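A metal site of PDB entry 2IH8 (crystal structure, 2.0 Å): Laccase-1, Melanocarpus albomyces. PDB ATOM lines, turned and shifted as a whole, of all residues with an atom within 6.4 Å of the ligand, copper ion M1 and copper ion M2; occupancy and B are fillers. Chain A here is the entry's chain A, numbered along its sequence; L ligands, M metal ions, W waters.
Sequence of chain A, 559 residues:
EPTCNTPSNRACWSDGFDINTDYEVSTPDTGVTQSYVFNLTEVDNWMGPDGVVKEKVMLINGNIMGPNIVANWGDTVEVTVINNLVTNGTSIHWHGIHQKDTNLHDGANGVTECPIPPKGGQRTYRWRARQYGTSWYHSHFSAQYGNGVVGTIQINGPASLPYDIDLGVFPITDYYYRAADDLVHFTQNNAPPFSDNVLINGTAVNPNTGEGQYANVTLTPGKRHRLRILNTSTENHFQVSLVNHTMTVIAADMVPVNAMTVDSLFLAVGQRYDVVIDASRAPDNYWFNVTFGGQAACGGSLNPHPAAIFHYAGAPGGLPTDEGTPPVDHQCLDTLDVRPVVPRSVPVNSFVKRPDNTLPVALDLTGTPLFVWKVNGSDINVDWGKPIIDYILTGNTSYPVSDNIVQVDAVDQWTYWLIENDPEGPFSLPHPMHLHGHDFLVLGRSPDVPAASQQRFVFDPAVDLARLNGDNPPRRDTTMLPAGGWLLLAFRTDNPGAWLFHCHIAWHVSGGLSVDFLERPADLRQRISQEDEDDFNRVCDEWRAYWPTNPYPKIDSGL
Copper ion M2 is bound by a ring nitrogen (ND1) of His 95 (1.9 Å), a ring nitrogen (NE2) of His 138 (2.0 Å), a ring nitrogen (NE2) of His 504 (2.0 Å) and an oxygen (O2) of the ligand (2.3 Å). Copper ion M2 has four donor atoms within binding distance.
His 93 touches copper ion M1 (CD2 to CU, 3.96 Å). CD2 of His 434 touches copper ion M1 (3.99 Å).
Copper ion M1 is bound by a ring nitrogen (NE2) of His 502, a ring nitrogen (NE2) of His 436, a ring nitrogen (NE2) of His 140 and an oxygen (O1) of the ligand.
NE2 of His 93 lies close to O2 of the ligand (3.3 Å). NE2 of His 434 lies close to O2 of the ligand, 3.3 Å away. Hydrophobic or aromatic side chains within 4 Å of the ligand: His 93, His 95, His 138, His 140, His 434, His 502 and His 504. Within 4 Å of the ligand: His 93, His 95, His 138, His 140, His 434, His 436, His 502 and His 504. The nearest printed residue that does not touch the ligand is Tyr 145 (5.9 Å).
Trp 136 touches copper ion M2 (CZ2 to CU, 3.7 Å). Four residues have an atom within 4 Å of copper ion M2: His 95, Trp 136, His 138 and His 504. The nearest printed residue that does not touch copper ion M2 is His 93 (4.02 Å).
N of His 93 sits at hydrogen-bond distance from O of His 138 (2.7 Å). N of His 434 is in hydrogen-bond range of O of His 502 (2.7 Å). A ring nitrogen (ND1) of His 436 lies within hydrogen-bond range of the side-chain carboxylate (OD2) of Asp 106 (2.7 Å). The chain-end carboxylate of Leu 559 is in hydrogen-bond range of a ring nitrogen (ND1) of His 140, at 2.9 Å. N of His 95 is in hydrogen-bond range of O of Trp 136 (2.9 Å). A ring nitrogen (NE2) of His 95 lies within hydrogen-bond range of the backbone carbonyl oxygen of Gly 270 (3.4 Å). A ring nitrogen (NE2) of His 95 lies close to a ring nitrogen (ND1) of His 434, at 3.4 Å. The backbone NH of His 436 sits at hydrogen-bond distance from the backbone carbonyl oxygen of Leu 500, 2.9 Å away.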
ATOM      1  N   HIS A  93     -20.080  25.515 -12.263  1.00  0.00           N
ATOM      2  CA  HIS A  93     -21.389  24.898 -12.393  1.00  0.00           C
ATOM      3  C   HIS A  93     -21.283  23.431 -12.030  1.00  0.00           C
ATOM      4  O   HIS A  93     -20.360  22.751 -12.444  1.00  0.00           O
ATOM      5  CB  HIS A  93     -21.937  25.078 -13.824  1.00  0.00           C
ATOM      6  CG  HIS A  93     -23.196  24.304 -14.088  1.00  0.00           C
ATOM      7  ND1 HIS A  93     -24.305  24.389 -13.281  1.00  0.00           N
ATOM      8  CD2 HIS A  93     -23.497  23.405 -15.047  1.00  0.00           C
ATOM      9  CE1 HIS A  93     -25.238  23.549 -13.725  1.00  0.00           C
ATOM     10  NE2 HIS A  93     -24.766  22.946 -14.802  1.00  0.00           N
ATOM     11  N   HIS A  95     -22.813  20.379 -12.813  1.00  0.00           N
ATOM     12  CA  HIS A  95     -23.576  19.678 -13.839  1.00  0.00           C
ATOM     13  C   HIS A  95     -24.196  18.374 -13.308  1.00  0.00           C
ATOM     14  O   HIS A  95     -23.480  17.442 -12.958  1.00  0.00           O
ATOM     15  CB  HIS A  95     -22.647  19.418 -15.034  1.00  0.00           C
ATOM     16  CG  HIS A  95     -23.334  18.888 -16.263  1.00  0.00           C
ATOM     17  ND1 HIS A  95     -23.141  19.440 -17.509  1.00  0.00           N
ATOM     18  CD2 HIS A  95     -24.135  17.812 -16.448  1.00  0.00           C
ATOM     19  CE1 HIS A  95     -23.794  18.727 -18.401  1.00  0.00           C
ATOM     20  NE2 HIS A  95     -24.406  17.732 -17.786  1.00  0.00           N
ATOM     21  N   GLY A  96     -25.517  18.307 -13.378  1.00  0.00           N
ATOM     22  CA  GLY A  96     -26.247  17.140 -12.925  1.00  0.00           C
ATOM     23  C   GLY A  96     -26.847  17.325 -11.549  1.00  0.00           C
ATOM     24  O   GLY A  96     -27.736  16.580 -11.148  1.00  0.00           O
ATOM     25  N   ASP A 106     -25.932  27.530  -8.520  1.00  0.00           N
ATOM     26  CA  ASP A 106     -25.831  26.821  -9.802  1.00  0.00           C
ATOM     27  C   ASP A 106     -24.539  27.088 -10.582  1.00  0.00           C
ATOM     28  O   ASP A 106     -24.107  26.245 -11.358  1.00  0.00           O
ATOM     29  CB  ASP A 106     -27.057  27.121 -10.661  1.00  0.00           C
ATOM     30  CG  ASP A 106     -27.198  26.171 -11.842  1.00  0.00           C
ATOM     31  OD1 ASP A 106     -27.165  24.941 -11.635  1.00  0.00           O
ATOM     32  OD2 ASP A 106     -27.329  26.671 -12.984  1.00  0.00           O
ATOM     33  N   ALA A 108     -24.003  29.548 -12.814  1.00  0.00           N
ATOM     34  CA  ALA A 108     -24.271  30.042 -14.164  1.00  0.00           C
ATOM     35  C   ALA A 108     -24.119  31.554 -14.150  1.00  0.00           C
ATOM     36  O   ALA A 108     -25.038  32.281 -13.772  1.00  0.00           O
ATOM     37  CB  ALA A 108     -25.682  29.641 -14.586  1.00  0.00           C
ATOM     38  N   TRP A 136     -20.415  15.944 -12.827  1.00  0.00           N
ATOM     39  CA  TRP A 136     -19.190  16.685 -13.004  1.00  0.00           C
ATOM     40  C   TRP A 136     -19.409  18.160 -12.805  1.00  0.00           C
ATOM     41  O   TRP A 136     -20.548  18.608 -12.634  1.00  0.00           O
ATOM     42  CB  TRP A 136     -18.552  16.395 -14.380  1.00  0.00           C
ATOM     43  CG  TRP A 136     -19.332  16.825 -15.607  1.00  0.00           C
ATOM     44  CD1 TRP A 136     -20.595  16.421 -15.961  1.00  0.00           C
ATOM     45  CD2 TRP A 136     -18.865  17.655 -16.667  1.00  0.00           C
ATOM     46  NE1 TRP A 136     -20.931  16.949 -17.194  1.00  0.00           N
ATOM     47  CE2 TRP A 136     -19.881  17.713 -17.652  1.00  0.00           C
ATOM     48  CE3 TRP A 136     -17.666  18.362 -16.885  1.00  0.00           C
ATOM     49  CZ2 TRP A 136     -19.742  18.438 -18.848  1.00  0.00           C
ATOM     50  CZ3 TRP A 136     -17.516  19.096 -18.101  1.00  0.00           C
ATOM     51  CH2 TRP A 136     -18.558  19.121 -19.066  1.00  0.00           C
ATOM     52  N   HIS A 138     -17.774  22.218 -13.895  1.00  0.00           N
ATOM     53  CA  HIS A 138     -17.008  22.980 -14.863  1.00  0.00           C
ATOM     54  C   HIS A 138     -17.333  24.456 -14.805  1.00  0.00           C
ATOM     55  O   HIS A 138     -18.380  24.851 -14.293  1.00  0.00           O
ATOM     56  CB  HIS A 138     -17.266  22.439 -16.291  1.00  0.00           C
ATOM     57  CG  HIS A 138     -18.695  22.549 -16.752  1.00  0.00           C
ATOM     58  ND1 HIS A 138     -19.217  23.707 -17.281  1.00  0.00           N
ATOM     59  CD2 HIS A 138     -19.696  21.636 -16.799  1.00  0.00           C
ATOM     60  CE1 HIS A 138     -20.471  23.503 -17.639  1.00  0.00           C
ATOM     61  NE2 HIS A 138     -20.786  22.250 -17.368  1.00  0.00           N
ATOM     62  N   SER A 139     -16.448  25.266 -15.369  1.00  0.00           N
ATOM     63  CA  SER A 139     -16.663  26.706 -15.431  1.00  0.00           C
ATOM     64  C   SER A 139     -17.748  26.968 -16.475  1.00  0.00           C
ATOM     65  O   SER A 139     -17.886  26.203 -17.433  1.00  0.00           O
ATOM     66  CB  SER A 139     -15.390  27.430 -15.843  1.00  0.00           C
ATOM     67  OG  SER A 139     -15.636  28.820 -16.027  1.00  0.00           O
ATOM     68  N   HIS A 140     -18.538  28.017 -16.228  1.00  0.00           N
ATOM     69  CA  HIS A 140     -19.570  28.422 -17.179  1.00  0.00           C
ATOM     70  C   HIS A 140     -19.223  29.814 -17.719  1.00  0.00           C
ATOM     71  O   HIS A 140     -20.059  30.481 -18.342  1.00  0.00           O
ATOM     72  CB  HIS A 140     -20.958  28.389 -16.539  1.00  0.00           C
ATOM     73  CG  HIS A 140     -21.983  27.659 -17.362  1.00  0.00           C
ATOM     74  ND1 HIS A 140     -22.189  27.919 -18.701  1.00  0.00           N
ATOM     75  CD2 HIS A 140     -22.845  26.665 -17.046  1.00  0.00           C
ATOM     76  CE1 HIS A 140     -23.118  27.117 -19.170  1.00  0.00           C
ATOM     77  NE2 HIS A 140     -23.538  26.339 -18.180  1.00  0.00           N
ATOM     78  N   TYR A 145     -13.855  26.240 -19.400  1.00  0.00           N
ATOM     79  CA  TYR A 145     -13.645  24.861 -18.979  1.00  0.00           C
ATOM     80  C   TYR A 145     -12.779  24.068 -19.962  1.00  0.00           C
ATOM     81  O   TYR A 145     -12.162  23.072 -19.600  1.00  0.00           O
ATOM     82  CB  TYR A 145     -14.961  24.162 -18.608  1.00  0.00           C
ATOM     83  CG  TYR A 145     -15.785  23.487 -19.699  1.00  0.00           C
ATOM     84  CD1 TYR A 145     -15.524  22.148 -20.082  1.00  0.00           C
ATOM     85  CD2 TYR A 145     -16.914  24.124 -20.257  1.00  0.00           C
ATOM     86  CE1 TYR A 145     -16.367  21.448 -20.990  1.00  0.00           C
ATOM     87  CE2 TYR A 145     -17.769  23.432 -21.167  1.00  0.00           C
ATOM     88  CZ  TYR A 145     -17.484  22.103 -21.527  1.00  0.00           C
ATOM     89  OH  TYR A 145     -18.294  21.417 -22.400  1.00  0.00           O
ATOM     90  N   GLY A 270     -21.181  16.004 -21.917  1.00  0.00           N
ATOM     91  CA  GLY A 270     -21.836  16.179 -20.642  1.00  0.00           C
ATOM     92  C   GLY A 270     -22.530  14.943 -20.092  1.00  0.00           C
ATOM     93  O   GLY A 270     -22.942  14.938 -18.935  1.00  0.00           O
ATOM     94  N   HIS A 434     -28.706  20.161 -22.893  1.00  0.00           N
ATOM     95  CA  HIS A 434     -28.596  20.010 -21.451  1.00  0.00           C
ATOM     96  C   HIS A 434     -29.473  21.000 -20.700  1.00  0.00           C
ATOM     97  O   HIS A 434     -29.542  22.174 -21.060  1.00  0.00           O
ATOM     98  CB  HIS A 434     -27.118  20.165 -21.037  1.00  0.00           C
ATOM     99  CG  HIS A 434     -26.907  20.243 -19.566  1.00  0.00           C
ATOM    100  ND1 HIS A 434     -27.327  19.256 -18.693  1.00  0.00           N
ATOM    101  CD2 HIS A 434     -26.371  21.220 -18.791  1.00  0.00           C
ATOM    102  CE1 HIS A 434     -27.068  19.629 -17.457  1.00  0.00           C
ATOM    103  NE2 HIS A 434     -26.486  20.812 -17.488  1.00  0.00           N
ATOM    104  N   HIS A 436     -30.340  22.698 -16.846  1.00  0.00           N
ATOM    105  CA  HIS A 436     -29.891  22.961 -15.491  1.00  0.00           C
ATOM    106  C   HIS A 436     -31.077  22.791 -14.542  1.00  0.00           C
ATOM    107  O   HIS A 436     -32.236  22.990 -14.935  1.00  0.00           O
ATOM    108  CB  HIS A 436     -29.386  24.416 -15.346  1.00  0.00           C
ATOM    109  CG  HIS A 436     -28.064  24.694 -15.989  1.00  0.00           C
ATOM    110  ND1 HIS A 436     -27.202  25.651 -15.491  1.00  0.00           N
ATOM    111  CD2 HIS A 436     -27.470  24.207 -17.111  1.00  0.00           C
ATOM    112  CE1 HIS A 436     -26.143  25.744 -16.279  1.00  0.00           C
ATOM    113  NE2 HIS A 436     -26.290  24.868 -17.265  1.00  0.00           N
ATOM    114  N   LEU A 500     -30.685  27.463 -17.190  1.00  0.00           N
ATOM    115  CA  LEU A 500     -30.221  27.391 -18.563  1.00  0.00           C
ATOM    116  C   LEU A 500     -30.530  26.053 -19.211  1.00  0.00           C
ATOM    117  O   LEU A 500     -30.505  25.003 -18.558  1.00  0.00           O
ATOM    118  CB  LEU A 500     -28.715  27.623 -18.645  1.00  0.00           C
ATOM    119  CG  LEU A 500     -28.183  29.025 -18.365  1.00  0.00           C
ATOM    120  CD1 LEU A 500     -26.666  28.973 -18.419  1.00  0.00           C
ATOM    121  CD2 LEU A 500     -28.730  30.022 -19.369  1.00  0.00           C
ATOM    122  N   HIS A 502     -29.332  24.555 -22.684  1.00  0.00           N
ATOM    123  CA  HIS A 502     -28.409  24.803 -23.772  1.00  0.00           C
ATOM    124  C   HIS A 502     -27.746  23.606 -24.390  1.00  0.00           C
ATOM    125  O   HIS A 502     -27.740  22.516 -23.817  1.00  0.00           O
ATOM    126  CB  HIS A 502     -27.314  25.762 -23.295  1.00  0.00           C
ATOM    127  CG  HIS A 502     -26.473  25.236 -22.167  1.00  0.00           C
ATOM    128  ND1 HIS A 502     -25.255  24.633 -22.376  1.00  0.00           N
ATOM    129  CD2 HIS A 502     -26.658  25.257 -20.820  1.00  0.00           C
ATOM    130  CE1 HIS A 502     -24.716  24.311 -21.205  1.00  0.00           C
ATOM    131  NE2 HIS A 502     -25.546  24.679 -20.252  1.00  0.00           N
ATOM    132  N   HIS A 504     -24.512  21.657 -25.113  1.00  0.00           N
ATOM    133  CA  HIS A 504     -23.271  21.583 -24.352  1.00  0.00           C
ATOM    134  C   HIS A 504     -21.988  21.674 -25.172  1.00  0.00           C
ATOM    135  O   HIS A 504     -20.888  21.604 -24.611  1.00  0.00           O
ATOM    136  CB  HIS A 504     -23.257  20.391 -23.417  1.00  0.00           C
ATOM    137  CG  HIS A 504     -22.637  20.691 -22.087  1.00  0.00           C
ATOM    138  ND1 HIS A 504     -21.295  20.945 -21.935  1.00  0.00           N
ATOM    139  CD2 HIS A 504     -23.188  20.811 -20.859  1.00  0.00           C
ATOM    140  CE1 HIS A 504     -21.043  21.207 -20.666  1.00  0.00           C
ATOM    141  NE2 HIS A 504     -22.174  21.129 -19.985  1.00  0.00           N
ATOM    142  N   VAL A 509     -22.851  27.088 -27.472  1.00  0.00           N
ATOM    143  CA  VAL A 509     -23.421  27.882 -26.366  1.00  0.00           C
ATOM    144  C   VAL A 509     -22.744  29.257 -26.323  1.00  0.00           C
ATOM    145  O   VAL A 509     -23.385  30.262 -26.004  1.00  0.00           O
ATOM    146  CB  VAL A 509     -23.403  27.135 -24.976  1.00  0.00           C
ATOM    147  CG1 VAL A 509     -21.988  26.861 -24.476  1.00  0.00           C
ATOM    148  CG2 VAL A 509     -24.220  27.916 -23.952  1.00  0.00           C
ATOM    149  N   LEU A 559     -21.565  32.326 -21.817  1.00  0.00           N
ATOM    150  CA  LEU A 559     -21.917  31.020 -21.258  1.00  0.00           C
ATOM    151  C   LEU A 559     -21.137  29.868 -21.902  1.00  0.00           C
ATOM    152  O   LEU A 559     -20.591  30.083 -23.001  1.00  0.00           O
ATOM    153  CB  LEU A 559     -23.418  30.770 -21.408  1.00  0.00           C
ATOM    154  CG  LEU A 559     -24.386  31.755 -20.734  1.00  0.00           C
ATOM    155  CD1 LEU A 559     -25.793  31.475 -21.191  1.00  0.00           C
ATOM    156  CD2 LEU A 559     -24.272  31.703 -19.213  1.00  0.00           C
ATOM    157  OXT LEU A 559     -21.084  28.776 -21.290  1.00  0.00           O
HETATM  158  O1  LIG L   1     -23.136  23.390 -18.770  1.00  0.00           O
HETATM  159  O2  LIG L   1     -23.839  22.677 -17.971  1.00  0.00           O
HETATM  160 CU    CU M   1     -24.790  24.870 -18.486  1.00  0.00          CU
HETATM  161 CU    CU M   2     -22.177  21.050 -18.030  1.00  0.00          CU
HETATM  162 CU    CU M   3     -25.549  21.862 -16.139  1.00  0.00          CU
HETATM  163  O   HOH W   1     -21.330  24.635 -20.845  1.00  0.00           O
